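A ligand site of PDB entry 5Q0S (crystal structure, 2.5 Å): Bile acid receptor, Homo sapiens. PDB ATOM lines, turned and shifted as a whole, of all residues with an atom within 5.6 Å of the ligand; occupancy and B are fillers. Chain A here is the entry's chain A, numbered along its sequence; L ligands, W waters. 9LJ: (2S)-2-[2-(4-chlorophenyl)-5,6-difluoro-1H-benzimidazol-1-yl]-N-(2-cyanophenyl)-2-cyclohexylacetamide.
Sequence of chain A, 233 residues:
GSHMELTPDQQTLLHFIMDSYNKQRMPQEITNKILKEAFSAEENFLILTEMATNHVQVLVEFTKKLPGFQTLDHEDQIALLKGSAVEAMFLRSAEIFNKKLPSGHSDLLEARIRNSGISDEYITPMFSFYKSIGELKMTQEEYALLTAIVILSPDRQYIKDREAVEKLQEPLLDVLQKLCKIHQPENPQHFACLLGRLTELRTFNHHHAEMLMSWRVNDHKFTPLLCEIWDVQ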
ATOM      1  N   ILE A  30      22.065  -5.592  10.256  1.00  0.00           N
ATOM      2  CA  ILE A  30      21.842  -5.190   8.864  1.00  0.00           C
ATOM      3  C   ILE A  30      23.002  -5.641   7.943  1.00  0.00           C
ATOM      4  O   ILE A  30      22.756  -6.290   6.920  1.00  0.00           O
ATOM      5  CB  ILE A  30      21.552  -3.657   8.796  1.00  0.00           C
ATOM      6  CG1 ILE A  30      20.381  -3.277   9.737  1.00  0.00           C
ATOM      7  CG2 ILE A  30      21.288  -3.165   7.364  1.00  0.00           C
ATOM      8  CD1 ILE A  30      20.586  -2.073  10.603  1.00  0.00           C
ATOM      9  N   THR A  31      24.255  -5.282   8.301  1.00  0.00           N
ATOM     10  CA  THR A  31      25.466  -5.599   7.536  1.00  0.00           C
ATOM     11  C   THR A  31      25.740  -7.106   7.472  1.00  0.00           C
ATOM     12  O   THR A  31      26.190  -7.576   6.426  1.00  0.00           O
ATOM     13  CB  THR A  31      26.686  -4.806   8.020  1.00  0.00           C
ATOM     14  OG1 THR A  31      26.786  -4.893   9.439  1.00  0.00           O
ATOM     15  CG2 THR A  31      26.633  -3.367   7.583  1.00  0.00           C
ATOM     16  N   ILE A  34      23.420  -8.568   4.650  1.00  0.00           N
ATOM     17  CA  ILE A  34      23.900  -8.159   3.331  1.00  0.00           C
ATOM     18  C   ILE A  34      25.166  -8.929   2.942  1.00  0.00           C
ATOM     19  O   ILE A  34      25.238  -9.456   1.833  1.00  0.00           O
ATOM     20  CB  ILE A  34      24.053  -6.618   3.210  1.00  0.00           C
ATOM     21  CG1 ILE A  34      22.709  -5.890   3.484  1.00  0.00           C
ATOM     22  CG2 ILE A  34      24.631  -6.187   1.843  1.00  0.00           C
ATOM     23  CD1 ILE A  34      22.848  -4.417   3.924  1.00  0.00           C
ATOM     24  N   ASN A  44      16.099  -8.210  -2.211  1.00  0.00           N
ATOM     25  CA  ASN A  44      16.658  -6.970  -1.643  1.00  0.00           C
ATOM     26  C   ASN A  44      15.623  -5.884  -1.462  1.00  0.00           C
ATOM     27  O   ASN A  44      15.629  -5.211  -0.416  1.00  0.00           O
ATOM     28  CB  ASN A  44      17.826  -6.467  -2.475  1.00  0.00           C
ATOM     29  CG  ASN A  44      19.122  -7.175  -2.195  1.00  0.00           C
ATOM     30  OD1 ASN A  44      19.427  -7.559  -1.046  1.00  0.00           O
ATOM     31  ND2 ASN A  44      19.929  -7.354  -3.239  1.00  0.00           N
ATOM     32  N   PHE A  45      14.727  -5.713  -2.470  1.00  0.00           N
ATOM     33  CA  PHE A  45      13.645  -4.730  -2.411  1.00  0.00           C
ATOM     34  C   PHE A  45      12.750  -5.027  -1.206  1.00  0.00           C
ATOM     35  O   PHE A  45      12.314  -4.102  -0.521  1.00  0.00           O
ATOM     36  CB  PHE A  45      12.825  -4.738  -3.707  1.00  0.00           C
ATOM     37  CG  PHE A  45      11.731  -3.699  -3.746  1.00  0.00           C
ATOM     38  CD1 PHE A  45      12.036  -2.366  -3.989  1.00  0.00           C
ATOM     39  CD2 PHE A  45      10.413  -4.042  -3.504  1.00  0.00           C
ATOM     40  CE1 PHE A  45      11.025  -1.400  -4.011  1.00  0.00           C
ATOM     41  CE2 PHE A  45       9.408  -3.070  -3.515  1.00  0.00           C
ATOM     42  CZ  PHE A  45       9.725  -1.767  -3.765  1.00  0.00           C
ATOM     43  N   ILE A  47      13.813  -6.773   1.553  1.00  0.00           N
ATOM     44  CA  ILE A  47      14.676  -6.521   2.721  1.00  0.00           C
ATOM     45  C   ILE A  47      14.590  -5.033   3.055  1.00  0.00           C
ATOM     46  O   ILE A  47      14.366  -4.687   4.215  1.00  0.00           O
ATOM     47  CB  ILE A  47      16.163  -7.021   2.472  1.00  0.00           C
ATOM     48  CG1 ILE A  47      16.251  -8.555   2.541  1.00  0.00           C
ATOM     49  CG2 ILE A  47      17.172  -6.384   3.429  1.00  0.00           C
ATOM     50  CD1 ILE A  47      17.392  -9.204   1.762  1.00  0.00           C
ATOM     51  N   LEU A  48      14.675  -4.158   1.999  1.00  0.00           N
ATOM     52  CA  LEU A  48      14.594  -2.691   2.091  1.00  0.00           C
ATOM     53  C   LEU A  48      13.298  -2.204   2.713  1.00  0.00           C
ATOM     54  O   LEU A  48      13.348  -1.365   3.612  1.00  0.00           O
ATOM     55  CB  LEU A  48      14.809  -2.045   0.703  1.00  0.00           C
ATOM     56  CG  LEU A  48      14.621  -0.512   0.589  1.00  0.00           C
ATOM     57  CD1 LEU A  48      15.792   0.234   1.153  1.00  0.00           C
ATOM     58  CD2 LEU A  48      14.437  -0.095  -0.851  1.00  0.00           C
ATOM     59  N   MET A  51      13.086  -3.228   6.361  1.00  0.00           N
ATOM     60  CA  MET A  51      14.076  -2.394   7.061  1.00  0.00           C
ATOM     61  C   MET A  51      13.503  -1.018   7.296  1.00  0.00           C
ATOM     62  O   MET A  51      13.524  -0.526   8.430  1.00  0.00           O
ATOM     63  CB  MET A  51      15.385  -2.275   6.251  1.00  0.00           C
ATOM     64  CG  MET A  51      16.339  -3.441   6.430  1.00  0.00           C
ATOM     65  SD  MET A  51      16.996  -3.678   8.080  1.00  0.00           S
ATOM     66  CE  MET A  51      17.610  -2.088   8.397  1.00  0.00           C
ATOM     67  N   ALA A  52      12.969  -0.408   6.227  1.00  0.00           N
ATOM     68  CA  ALA A  52      12.379   0.924   6.254  1.00  0.00           C
ATOM     69  C   ALA A  52      11.124   1.026   7.097  1.00  0.00           C
ATOM     70  O   ALA A  52      10.926   2.075   7.700  1.00  0.00           O
ATOM     71  CB  ALA A  52      12.132   1.408   4.846  1.00  0.00           C
ATOM     72  N   HIS A  55      12.307   0.964  10.722  1.00  0.00           N
ATOM     73  CA  HIS A  55      12.941   2.258  10.913  1.00  0.00           C
ATOM     74  C   HIS A  55      11.936   3.350  11.255  1.00  0.00           C
ATOM     75  O   HIS A  55      12.152   4.104  12.222  1.00  0.00           O
ATOM     76  CB  HIS A  55      13.775   2.673   9.680  1.00  0.00           C
ATOM     77  CG  HIS A  55      14.413   4.012   9.834  1.00  0.00           C
ATOM     78  ND1 HIS A  55      15.573   4.181  10.595  1.00  0.00           N
ATOM     79  CD2 HIS A  55      14.007   5.228   9.380  1.00  0.00           C
ATOM     80  CE1 HIS A  55      15.853   5.478  10.549  1.00  0.00           C
ATOM     81  NE2 HIS A  55      14.932   6.146   9.850  1.00  0.00           N
ATOM     82  N   MET A  89      16.436   8.011   7.511  1.00  0.00           N
ATOM     83  CA  MET A  89      16.809   6.682   7.049  1.00  0.00           C
ATOM     84  C   MET A  89      18.168   6.707   6.348  1.00  0.00           C
ATOM     85  O   MET A  89      18.999   5.841   6.625  1.00  0.00           O
ATOM     86  CB  MET A  89      15.722   6.081   6.148  1.00  0.00           C
ATOM     87  CG  MET A  89      16.137   4.788   5.517  1.00  0.00           C
ATOM     88  SD  MET A  89      15.591   4.442   3.822  1.00  0.00           S
ATOM     89  CE  MET A  89      15.849   5.983   3.053  1.00  0.00           C
ATOM     90  N   PHE A  90      18.402   7.705   5.465  1.00  0.00           N
ATOM     91  CA  PHE A  90      19.671   7.830   4.764  1.00  0.00           C
ATOM     92  C   PHE A  90      20.807   8.205   5.697  1.00  0.00           C
ATOM     93  O   PHE A  90      21.926   7.735   5.501  1.00  0.00           O
ATOM     94  CB  PHE A  90      19.573   8.801   3.578  1.00  0.00           C
ATOM     95  CG  PHE A  90      18.923   8.211   2.350  1.00  0.00           C
ATOM     96  CD1 PHE A  90      19.517   7.150   1.669  1.00  0.00           C
ATOM     97  CD2 PHE A  90      17.740   8.734   1.856  1.00  0.00           C
ATOM     98  CE1 PHE A  90      18.928   6.610   0.532  1.00  0.00           C
ATOM     99  CE2 PHE A  90      17.148   8.202   0.698  1.00  0.00           C
ATOM    100  CZ  PHE A  90      17.747   7.126   0.059  1.00  0.00           C
ATOM    101  N   ARG A  92      20.999   7.299   8.864  1.00  0.00           N
ATOM    102  CA  ARG A  92      21.188   6.027   9.564  1.00  0.00           C
ATOM    103  C   ARG A  92      21.950   5.020   8.709  1.00  0.00           C
ATOM    104  O   ARG A  92      22.811   4.311   9.228  1.00  0.00           O
ATOM    105  CB  ARG A  92      19.825   5.439  10.026  1.00  0.00           C
ATOM    106  CG  ARG A  92      19.884   4.155  10.838  1.00  0.00           C
ATOM    107  CD  ARG A  92      20.869   4.190  12.004  1.00  0.00           C
ATOM    108  NE  ARG A  92      20.814   2.978  12.807  1.00  0.00           N
ATOM    109  CZ  ARG A  92      21.557   2.769  13.883  1.00  0.00           C
ATOM    110  NH1 ARG A  92      22.437   3.673  14.277  1.00  0.00           N
ATOM    111  NH2 ARG A  92      21.430   1.641  14.577  1.00  0.00           N
ATOM    112  N   SER A  93      21.641   4.964   7.394  1.00  0.00           N
ATOM    113  CA  SER A  93      22.296   4.082   6.406  1.00  0.00           C
ATOM    114  C   SER A  93      23.743   4.516   6.222  1.00  0.00           C
ATOM    115  O   SER A  93      24.622   3.662   6.124  1.00  0.00           O
ATOM    116  CB  SER A  93      21.543   4.105   5.074  1.00  0.00           C
ATOM    117  OG  SER A  93      20.270   3.513   5.203  1.00  0.00           O
ATOM    118  N   ALA A  94      23.994   5.847   6.234  1.00  0.00           N
ATOM    119  CA  ALA A  94      25.321   6.455   6.175  1.00  0.00           C
ATOM    120  C   ALA A  94      26.130   6.077   7.422  1.00  0.00           C
ATOM    121  O   ALA A  94      27.281   5.687   7.297  1.00  0.00           O
ATOM    122  CB  ALA A  94      25.210   7.963   6.062  1.00  0.00           C
ATOM    123  N   ILE A  96      25.607   3.357   9.501  1.00  0.00           N
ATOM    124  CA  ILE A  96      25.844   1.911   9.359  1.00  0.00           C
ATOM    125  C   ILE A  96      26.964   1.645   8.369  1.00  0.00           C
ATOM    126  O   ILE A  96      27.877   0.886   8.693  1.00  0.00           O
ATOM    127  CB  ILE A  96      24.531   1.121   9.031  1.00  0.00           C
ATOM    128  CG1 ILE A  96      23.548   1.175  10.214  1.00  0.00           C
ATOM    129  CG2 ILE A  96      24.830  -0.333   8.662  1.00  0.00           C
ATOM    130  CD1 ILE A  96      22.126   1.159   9.836  1.00  0.00           C
ATOM    131  N   PHE A  97      26.932   2.330   7.207  1.00  0.00           N
ATOM    132  CA  PHE A  97      27.945   2.229   6.151  1.00  0.00           C
ATOM    133  C   PHE A  97      29.354   2.514   6.641  1.00  0.00           C
ATOM    134  O   PHE A  97      30.288   1.833   6.225  1.00  0.00           O
ATOM    135  CB  PHE A  97      27.608   3.189   5.000  1.00  0.00           C
ATOM    136  CG  PHE A  97      28.424   3.008   3.745  1.00  0.00           C
ATOM    137  CD1 PHE A  97      28.066   2.051   2.799  1.00  0.00           C
ATOM    138  CD2 PHE A  97      29.534   3.811   3.491  1.00  0.00           C
ATOM    139  CE1 PHE A  97      28.822   1.873   1.637  1.00  0.00           C
ATOM    140  CE2 PHE A  97      30.279   3.647   2.317  1.00  0.00           C
ATOM    141  CZ  PHE A  97      29.915   2.681   1.397  1.00  0.00           C
ATOM    142  N   ASN A  98      29.500   3.518   7.511  1.00  0.00           N
ATOM    143  CA  ASN A  98      30.800   3.980   7.991  1.00  0.00           C
ATOM    144  C   ASN A  98      31.264   3.312   9.292  1.00  0.00           C
ATOM    145  O   ASN A  98      32.314   3.693   9.827  1.00  0.00           O
ATOM    146  CB  ASN A  98      30.816   5.491   8.097  1.00  0.00           C
ATOM    147  CG  ASN A  98      30.731   6.153   6.732  1.00  0.00           C
ATOM    148  OD1 ASN A  98      31.640   6.047   5.888  1.00  0.00           O
ATOM    149  ND2 ASN A  98      29.638   6.841   6.483  1.00  0.00           N
ATOM    150  N   LEU A 109      30.339  -4.974   1.158  1.00  0.00           N
ATOM    151  CA  LEU A 109      29.075  -4.338   1.532  1.00  0.00           C
ATOM    152  C   LEU A 109      28.658  -3.318   0.460  1.00  0.00           C
ATOM    153  O   LEU A 109      27.530  -3.384  -0.053  1.00  0.00           O
ATOM    154  CB  LEU A 109      29.220  -3.646   2.898  1.00  0.00           C
ATOM    155  CG  LEU A 109      28.014  -2.838   3.412  1.00  0.00           C
ATOM    156  CD1 LEU A 109      26.845  -3.751   3.806  1.00  0.00           C
ATOM    157  CD2 LEU A 109      28.425  -1.911   4.527  1.00  0.00           C
ATOM    158  N   ARG A 112      27.757  -5.095  -2.798  1.00  0.00           N
ATOM    159  CA  ARG A 112      26.458  -5.755  -2.652  1.00  0.00           C
ATOM    160  C   ARG A 112      25.332  -4.739  -2.804  1.00  0.00           C
ATOM    161  O   ARG A 112      24.430  -4.992  -3.600  1.00  0.00           O
ATOM    162  CB  ARG A 112      26.362  -6.535  -1.321  1.00  0.00           C
ATOM    163  CG  ARG A 112      27.178  -7.840  -1.304  1.00  0.00           C
ATOM    164  CD  ARG A 112      26.371  -9.079  -1.659  1.00  0.00           C
ATOM    165  NE  ARG A 112      27.207 -10.275  -1.806  1.00  0.00           N
ATOM    166  CZ  ARG A 112      27.626 -11.022  -0.786  1.00  0.00           C
ATOM    167  NH1 ARG A 112      28.367 -12.100  -1.013  1.00  0.00           N
ATOM    168  NH2 ARG A 112      27.327 -10.692   0.459  1.00  0.00           N
ATOM    169  N   ILE A 113      25.406  -3.563  -2.113  1.00  0.00           N
ATOM    170  CA  ILE A 113      24.432  -2.447  -2.207  1.00  0.00           C
ATOM    171  C   ILE A 113      24.392  -1.908  -3.649  1.00  0.00           C
ATOM    172  O   ILE A 113      23.312  -1.695  -4.179  1.00  0.00           O
ATOM    173  CB  ILE A 113      24.687  -1.323  -1.150  1.00  0.00           C
ATOM    174  CG1 ILE A 113      24.633  -1.849   0.299  1.00  0.00           C
ATOM    175  CG2 ILE A 113      23.695  -0.150  -1.312  1.00  0.00           C
ATOM    176  CD1 ILE A 113      25.441  -1.039   1.271  1.00  0.00           C
ATOM    177  N   SER A 116      22.117  -4.129  -5.705  1.00  0.00           N
ATOM    178  CA  SER A 116      20.907  -4.514  -4.964  1.00  0.00           C
ATOM    179  C   SER A 116      19.615  -4.445  -5.812  1.00  0.00           C
ATOM    180  O   SER A 116      18.612  -5.063  -5.433  1.00  0.00           O
ATOM    181  CB  SER A 116      20.779  -3.693  -3.691  1.00  0.00           C
ATOM    182  OG  SER A 116      20.653  -2.301  -3.954  1.00  0.00           O
ATOM    183  N   ILE A 118      18.733  -1.190  -7.392  1.00  0.00           N
ATOM    184  CA  ILE A 118      18.621   0.250  -7.582  1.00  0.00           C
ATOM    185  C   ILE A 118      19.429   0.663  -8.836  1.00  0.00           C
ATOM    186  O   ILE A 118      20.461   0.047  -9.117  1.00  0.00           O
ATOM    187  CB  ILE A 118      19.059   0.986  -6.290  1.00  0.00           C
ATOM    188  CG1 ILE A 118      18.968   2.530  -6.417  1.00  0.00           C
ATOM    189  CG2 ILE A 118      20.455   0.525  -5.820  1.00  0.00           C
ATOM    190  CD1 ILE A 118      19.038   3.300  -5.110  1.00  0.00           C
ATOM    191  N   MET A 126      24.294   8.679  -3.797  1.00  0.00           N
ATOM    192  CA  MET A 126      24.122   7.957  -2.532  1.00  0.00           C
ATOM    193  C   MET A 126      25.445   7.577  -1.891  1.00  0.00           C
ATOM    194  O   MET A 126      25.609   7.756  -0.696  1.00  0.00           O
ATOM    195  CB  MET A 126      23.224   6.725  -2.744  1.00  0.00           C
ATOM    196  CG  MET A 126      22.758   6.062  -1.455  1.00  0.00           C
ATOM    197  SD  MET A 126      22.088   4.411  -1.744  1.00  0.00           S
ATOM    198  CE  MET A 126      23.527   3.521  -2.082  1.00  0.00           C
ATOM    199  N   TYR A 130      27.373   9.105   1.615  1.00  0.00           N
ATOM    200  CA  TYR A 130      27.836   8.137   2.623  1.00  0.00           C
ATOM    201  C   TYR A 130      29.302   8.347   2.955  1.00  0.00           C
ATOM    202  O   TYR A 130      29.683   8.364   4.127  1.00  0.00           O
ATOM    203  CB  TYR A 130      27.612   6.680   2.147  1.00  0.00           C
ATOM    204  CG  TYR A 130      26.178   6.196   2.110  1.00  0.00           C
ATOM    205  CD1 TYR A 130      25.139   7.002   2.546  1.00  0.00           C
ATOM    206  CD2 TYR A 130      25.873   4.924   1.633  1.00  0.00           C
ATOM    207  CE1 TYR A 130      23.817   6.556   2.508  1.00  0.00           C
ATOM    208  CE2 TYR A 130      24.552   4.480   1.558  1.00  0.00           C
ATOM    209  CZ  TYR A 130      23.524   5.299   2.016  1.00  0.00           C
ATOM    210  OH  TYR A 130      22.210   4.901   1.928  1.00  0.00           O
ATOM    211  N   MET A 211      13.733   6.720  -6.955  1.00  0.00           N
ATOM    212  CA  MET A 211      14.769   5.808  -6.481  1.00  0.00           C
ATOM    213  C   MET A 211      14.203   4.420  -6.231  1.00  0.00           C
ATOM    214  O   MET A 211      14.813   3.432  -6.639  1.00  0.00           O
ATOM    215  CB  MET A 211      15.390   6.368  -5.193  1.00  0.00           C
ATOM    216  CG  MET A 211      16.868   6.179  -5.086  1.00  0.00           C
ATOM    217  SD  MET A 211      17.650   6.951  -3.638  1.00  0.00           S
ATOM    218  CE  MET A 211      17.636   8.661  -4.127  1.00  0.00           C
ATOM    219  N   LEU A 212      13.017   4.365  -5.587  1.00  0.00           N
ATOM    220  CA  LEU A 212      12.298   3.128  -5.235  1.00  0.00           C
ATOM    221  C   LEU A 212      11.608   2.504  -6.422  1.00  0.00           C
ATOM    222  O   LEU A 212      11.630   1.298  -6.553  1.00  0.00           O
ATOM    223  CB  LEU A 212      11.252   3.415  -4.161  1.00  0.00           C
ATOM    224  CG  LEU A 212      11.748   3.964  -2.828  1.00  0.00           C
ATOM    225  CD1 LEU A 212      10.631   4.731  -2.148  1.00  0.00           C
ATOM    226  CD2 LEU A 212      12.307   2.868  -1.949  1.00  0.00           C
ATOM    227  N   TRP A 215      13.845   0.604  -9.127  1.00  0.00           N
ATOM    228  CA  TRP A 215      14.384  -0.686  -8.692  1.00  0.00           C
ATOM    229  C   TRP A 215      14.039  -1.768  -9.708  1.00  0.00           C
ATOM    230  O   TRP A 215      12.889  -1.848 -10.148  1.00  0.00           O
ATOM    231  CB  TRP A 215      13.821  -1.036  -7.318  1.00  0.00           C
ATOM    232  CG  TRP A 215      14.732  -1.882  -6.475  1.00  0.00           C
ATOM    233  CD1 TRP A 215      14.887  -3.231  -6.549  1.00  0.00           C
ATOM    234  CD2 TRP A 215      15.577  -1.433  -5.412  1.00  0.00           C
ATOM    235  NE1 TRP A 215      15.789  -3.656  -5.604  1.00  0.00           N
ATOM    236  CE2 TRP A 215      16.227  -2.567  -4.893  1.00  0.00           C
ATOM    237  CE3 TRP A 215      15.843  -0.178  -4.851  1.00  0.00           C
ATOM    238  CZ2 TRP A 215      17.134  -2.481  -3.833  1.00  0.00           C
ATOM    239  CZ3 TRP A 215      16.729  -0.092  -3.788  1.00  0.00           C
ATOM    240  CH2 TRP A 215      17.383  -1.236  -3.301  1.00  0.00           C
ATOM    241  N   TRP A 230       6.476   7.933   2.539  1.00  0.00           N
ATOM    242  CA  TRP A 230       7.060   7.996   1.194  1.00  0.00           C
ATOM    243  C   TRP A 230       5.940   8.331   0.200  1.00  0.00           C
ATOM    244  O   TRP A 230       4.783   7.966   0.425  1.00  0.00           O
ATOM    245  CB  TRP A 230       7.680   6.654   0.797  1.00  0.00           C
ATOM    246  CG  TRP A 230       8.878   6.219   1.582  1.00  0.00           C
ATOM    247  CD1 TRP A 230       9.610   6.972   2.457  1.00  0.00           C
ATOM    248  CD2 TRP A 230       9.525   4.952   1.514  1.00  0.00           C
ATOM    249  NE1 TRP A 230      10.654   6.241   2.956  1.00  0.00           N
ATOM    250  CE2 TRP A 230      10.636   4.997   2.391  1.00  0.00           C
ATOM    251  CE3 TRP A 230       9.264   3.758   0.807  1.00  0.00           C
ATOM    252  CZ2 TRP A 230      11.521   3.924   2.525  1.00  0.00           C
ATOM    253  CZ3 TRP A 230      10.130   2.687   0.968  1.00  0.00           C
ATOM    254  CH2 TRP A 230      11.233   2.771   1.826  1.00  0.00           C
HETATM  255  C4  9LJ L   1      23.876   1.461   3.541  1.00  0.00           C
HETATM  256  C7  9LJ L   1      22.604   1.330   2.989  1.00  0.00           C
HETATM  257  C8  9LJ L   1      21.823   0.222   3.317  1.00  0.00           C
HETATM  258  C10 9LJ L   1      20.755   1.574   1.896  1.00  0.00           C
HETATM  259  C13 9LJ L   1      18.610   2.751   1.597  1.00  0.00           C
HETATM  260  C15 9LJ L   1      17.666   3.184  -0.545  1.00  0.00           C
HETATM  261  C17 9LJ L   1      19.759   2.034  -0.378  1.00  0.00           C
HETATM  262  C20 9LJ L   1      19.683  -1.876   1.982  1.00  0.00           C
HETATM  263  C21 9LJ L   1      18.754  -0.499   4.016  1.00  0.00           C
HETATM  264  C24 9LJ L   1      18.369  -2.540   1.536  1.00  0.00           C
HETATM  265  C26 9LJ L   1      19.547  -3.837  -0.272  1.00  0.00           C
HETATM  266  C28 9LJ L   1      20.655  -1.815   0.774  1.00  0.00           C
HETATM  267  C1  9LJ L   1      24.304   0.478   4.414  1.00  0.00           C
HETATM  268  C2  9LJ L   1      23.507  -0.621   4.719  1.00  0.00           C
HETATM  269  C3  9LJ L   1      22.250  -0.780   4.184  1.00  0.00           C
HETATM  270  N11 9LJ L   1      21.917   2.161   2.098  1.00  0.00           N
HETATM  271  N9  9LJ L   1      20.629   0.391   2.594  1.00  0.00           N
HETATM  272  C19 9LJ L   1      19.431  -0.482   2.576  1.00  0.00           C
HETATM  273  C25 9LJ L   1      18.600  -3.913   0.914  1.00  0.00           C
HETATM  274  C27 9LJ L   1      20.866  -3.202   0.134  1.00  0.00           C
HETATM  275  O23 9LJ L   1      18.127  -1.471   4.418  1.00  0.00           O
HETATM  276  N22 9LJ L   1      18.939   0.645   4.721  1.00  0.00           N
HETATM  277  C29 9LJ L   1      18.476   0.972   6.028  1.00  0.00           C
HETATM  278  C30 9LJ L   1      17.124   1.332   6.205  1.00  0.00           C
HETATM  279  C31 9LJ L   1      16.653   1.660   7.479  1.00  0.00           C
HETATM  280  C32 9LJ L   1      17.498   1.629   8.577  1.00  0.00           C
HETATM  281  C33 9LJ L   1      18.820   1.277   8.412  1.00  0.00           C
HETATM  282  C34 9LJ L   1      19.324   0.944   7.150  1.00  0.00           C
HETATM  283  C35 9LJ L   1      16.227   1.373   5.084  1.00  0.00           C
HETATM  284  N36 9LJ L   1      15.549   1.384   4.169  1.00  0.00           N
HETATM  285  C12 9LJ L   1      19.711   2.123   1.007  1.00  0.00           C
HETATM  286  C14 9LJ L   1      17.586   3.279   0.828  1.00  0.00           C
HETATM  287  C16 9LJ L   1      18.738   2.566  -1.161  1.00  0.00           C
HETATM  288 CL18 9LJ L   1      16.383   3.847  -1.516  1.00  0.00          CL
HETATM  289  F6  9LJ L   1      23.987  -1.557   5.574  1.00  0.00           F
HETATM  290  F5  9LJ L   1      25.522   0.570   4.964  1.00  0.00           F
HETATM  291  O   HOH W   1      16.571   1.094  11.800  1.00  0.00           O
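The side-chain hydroxyl (OH) of Tyr 130 is in hydrogen-bond range of a nitrogen (N11) of the ligand.
N22 of the ligand lies within hydrogen-bond range of OG of Ser 93, 3.2 Å away.
NE2 of His 55 lies within hydrogen-bond range of N of Met 89.
The side-chain amide nitrogen (ND2) of Asn 98 sits at hydrogen-bond distance from the backbone carbonyl oxygen (O) of Tyr 130, at 2.8 Å.
The side-chain sulfur (SD) of Met 126 sits close to the side-chain hydroxyl (OH) of Tyr 130, at 3.7 Å.
NE1 of Trp 215 is in hydrogen-bond range of O of Ser 116.
The backbone carbonyl oxygen of Ile 113 is in hydrogen-bond range of the side-chain hydroxyl of Ser 116 (2.7 Å).
O of Ser 116 lies close to ND2 of Asn 44, at 3.4 Å.
The backbone carbonyl oxygen (O) of Ile 34 sits at hydrogen-bond distance from the guanidinium group (NH2) of Arg 112, at 2.8 Å.
The backbone carbonyl oxygen (O) of Met 89 is in hydrogen-bond range of the side-chain hydroxyl (OG) of Ser 93, 3.0 Å away.
A nitrogen (N36) of the ligand sits close to the side-chain sulfur of Met 89 (3.1 Å).
The backbone NH (N) of Phe 97 sits close to a fluorine (F5) of the ligand (3.2 Å).
Ile 30 touches the ligand (CG2 to F6, 3.6 Å).
Thr 31 touches the ligand.
Ile 34 touches the ligand (CD1 to F6, 3.5 Å).
Asn 44 touches the ligand.
CG2 of Ile 47 touches C25 of the ligand (3.8 Å).
CD1 of Leu 48 touches N36 of the ligand, at 3.2 Å.
CG of Met 51 touches O23 of the ligand (3.3 Å).
CB of Ala 52 touches N36 of the ligand, 3.5 Å away.
His 55 touches the ligand.
CE1 of Phe 90 touches C14 of the ligand, 3.6 Å away.
Arg 92 touches the ligand (CG to C33, 3.9 Å).
CG2 of Ile 96 touches F6 of the ligand, 3.4 Å away.
Leu 109 touches the ligand.
Ile 113 touches the ligand (CD1 to C1, 3.7 Å).
CB of Ser 116 touches C26 of the ligand (3.6 Å).
Met 126 touches the ligand.
SD of Met 211 touches CL18 of the ligand, 3.97 Å away.
Hydrophobic or aromatic side chains that line the ligand: Ile 30, Ile 34, Ile 47, Leu 48, Met 51, Ala 52, His 55, Met 89, Phe 90, Ile 96, Phe 97, Leu 109, Ile 113, Met 126, Tyr 130 and Met 211.
Of the 29 residues printed, 21 come within 4 Å of the ligand.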
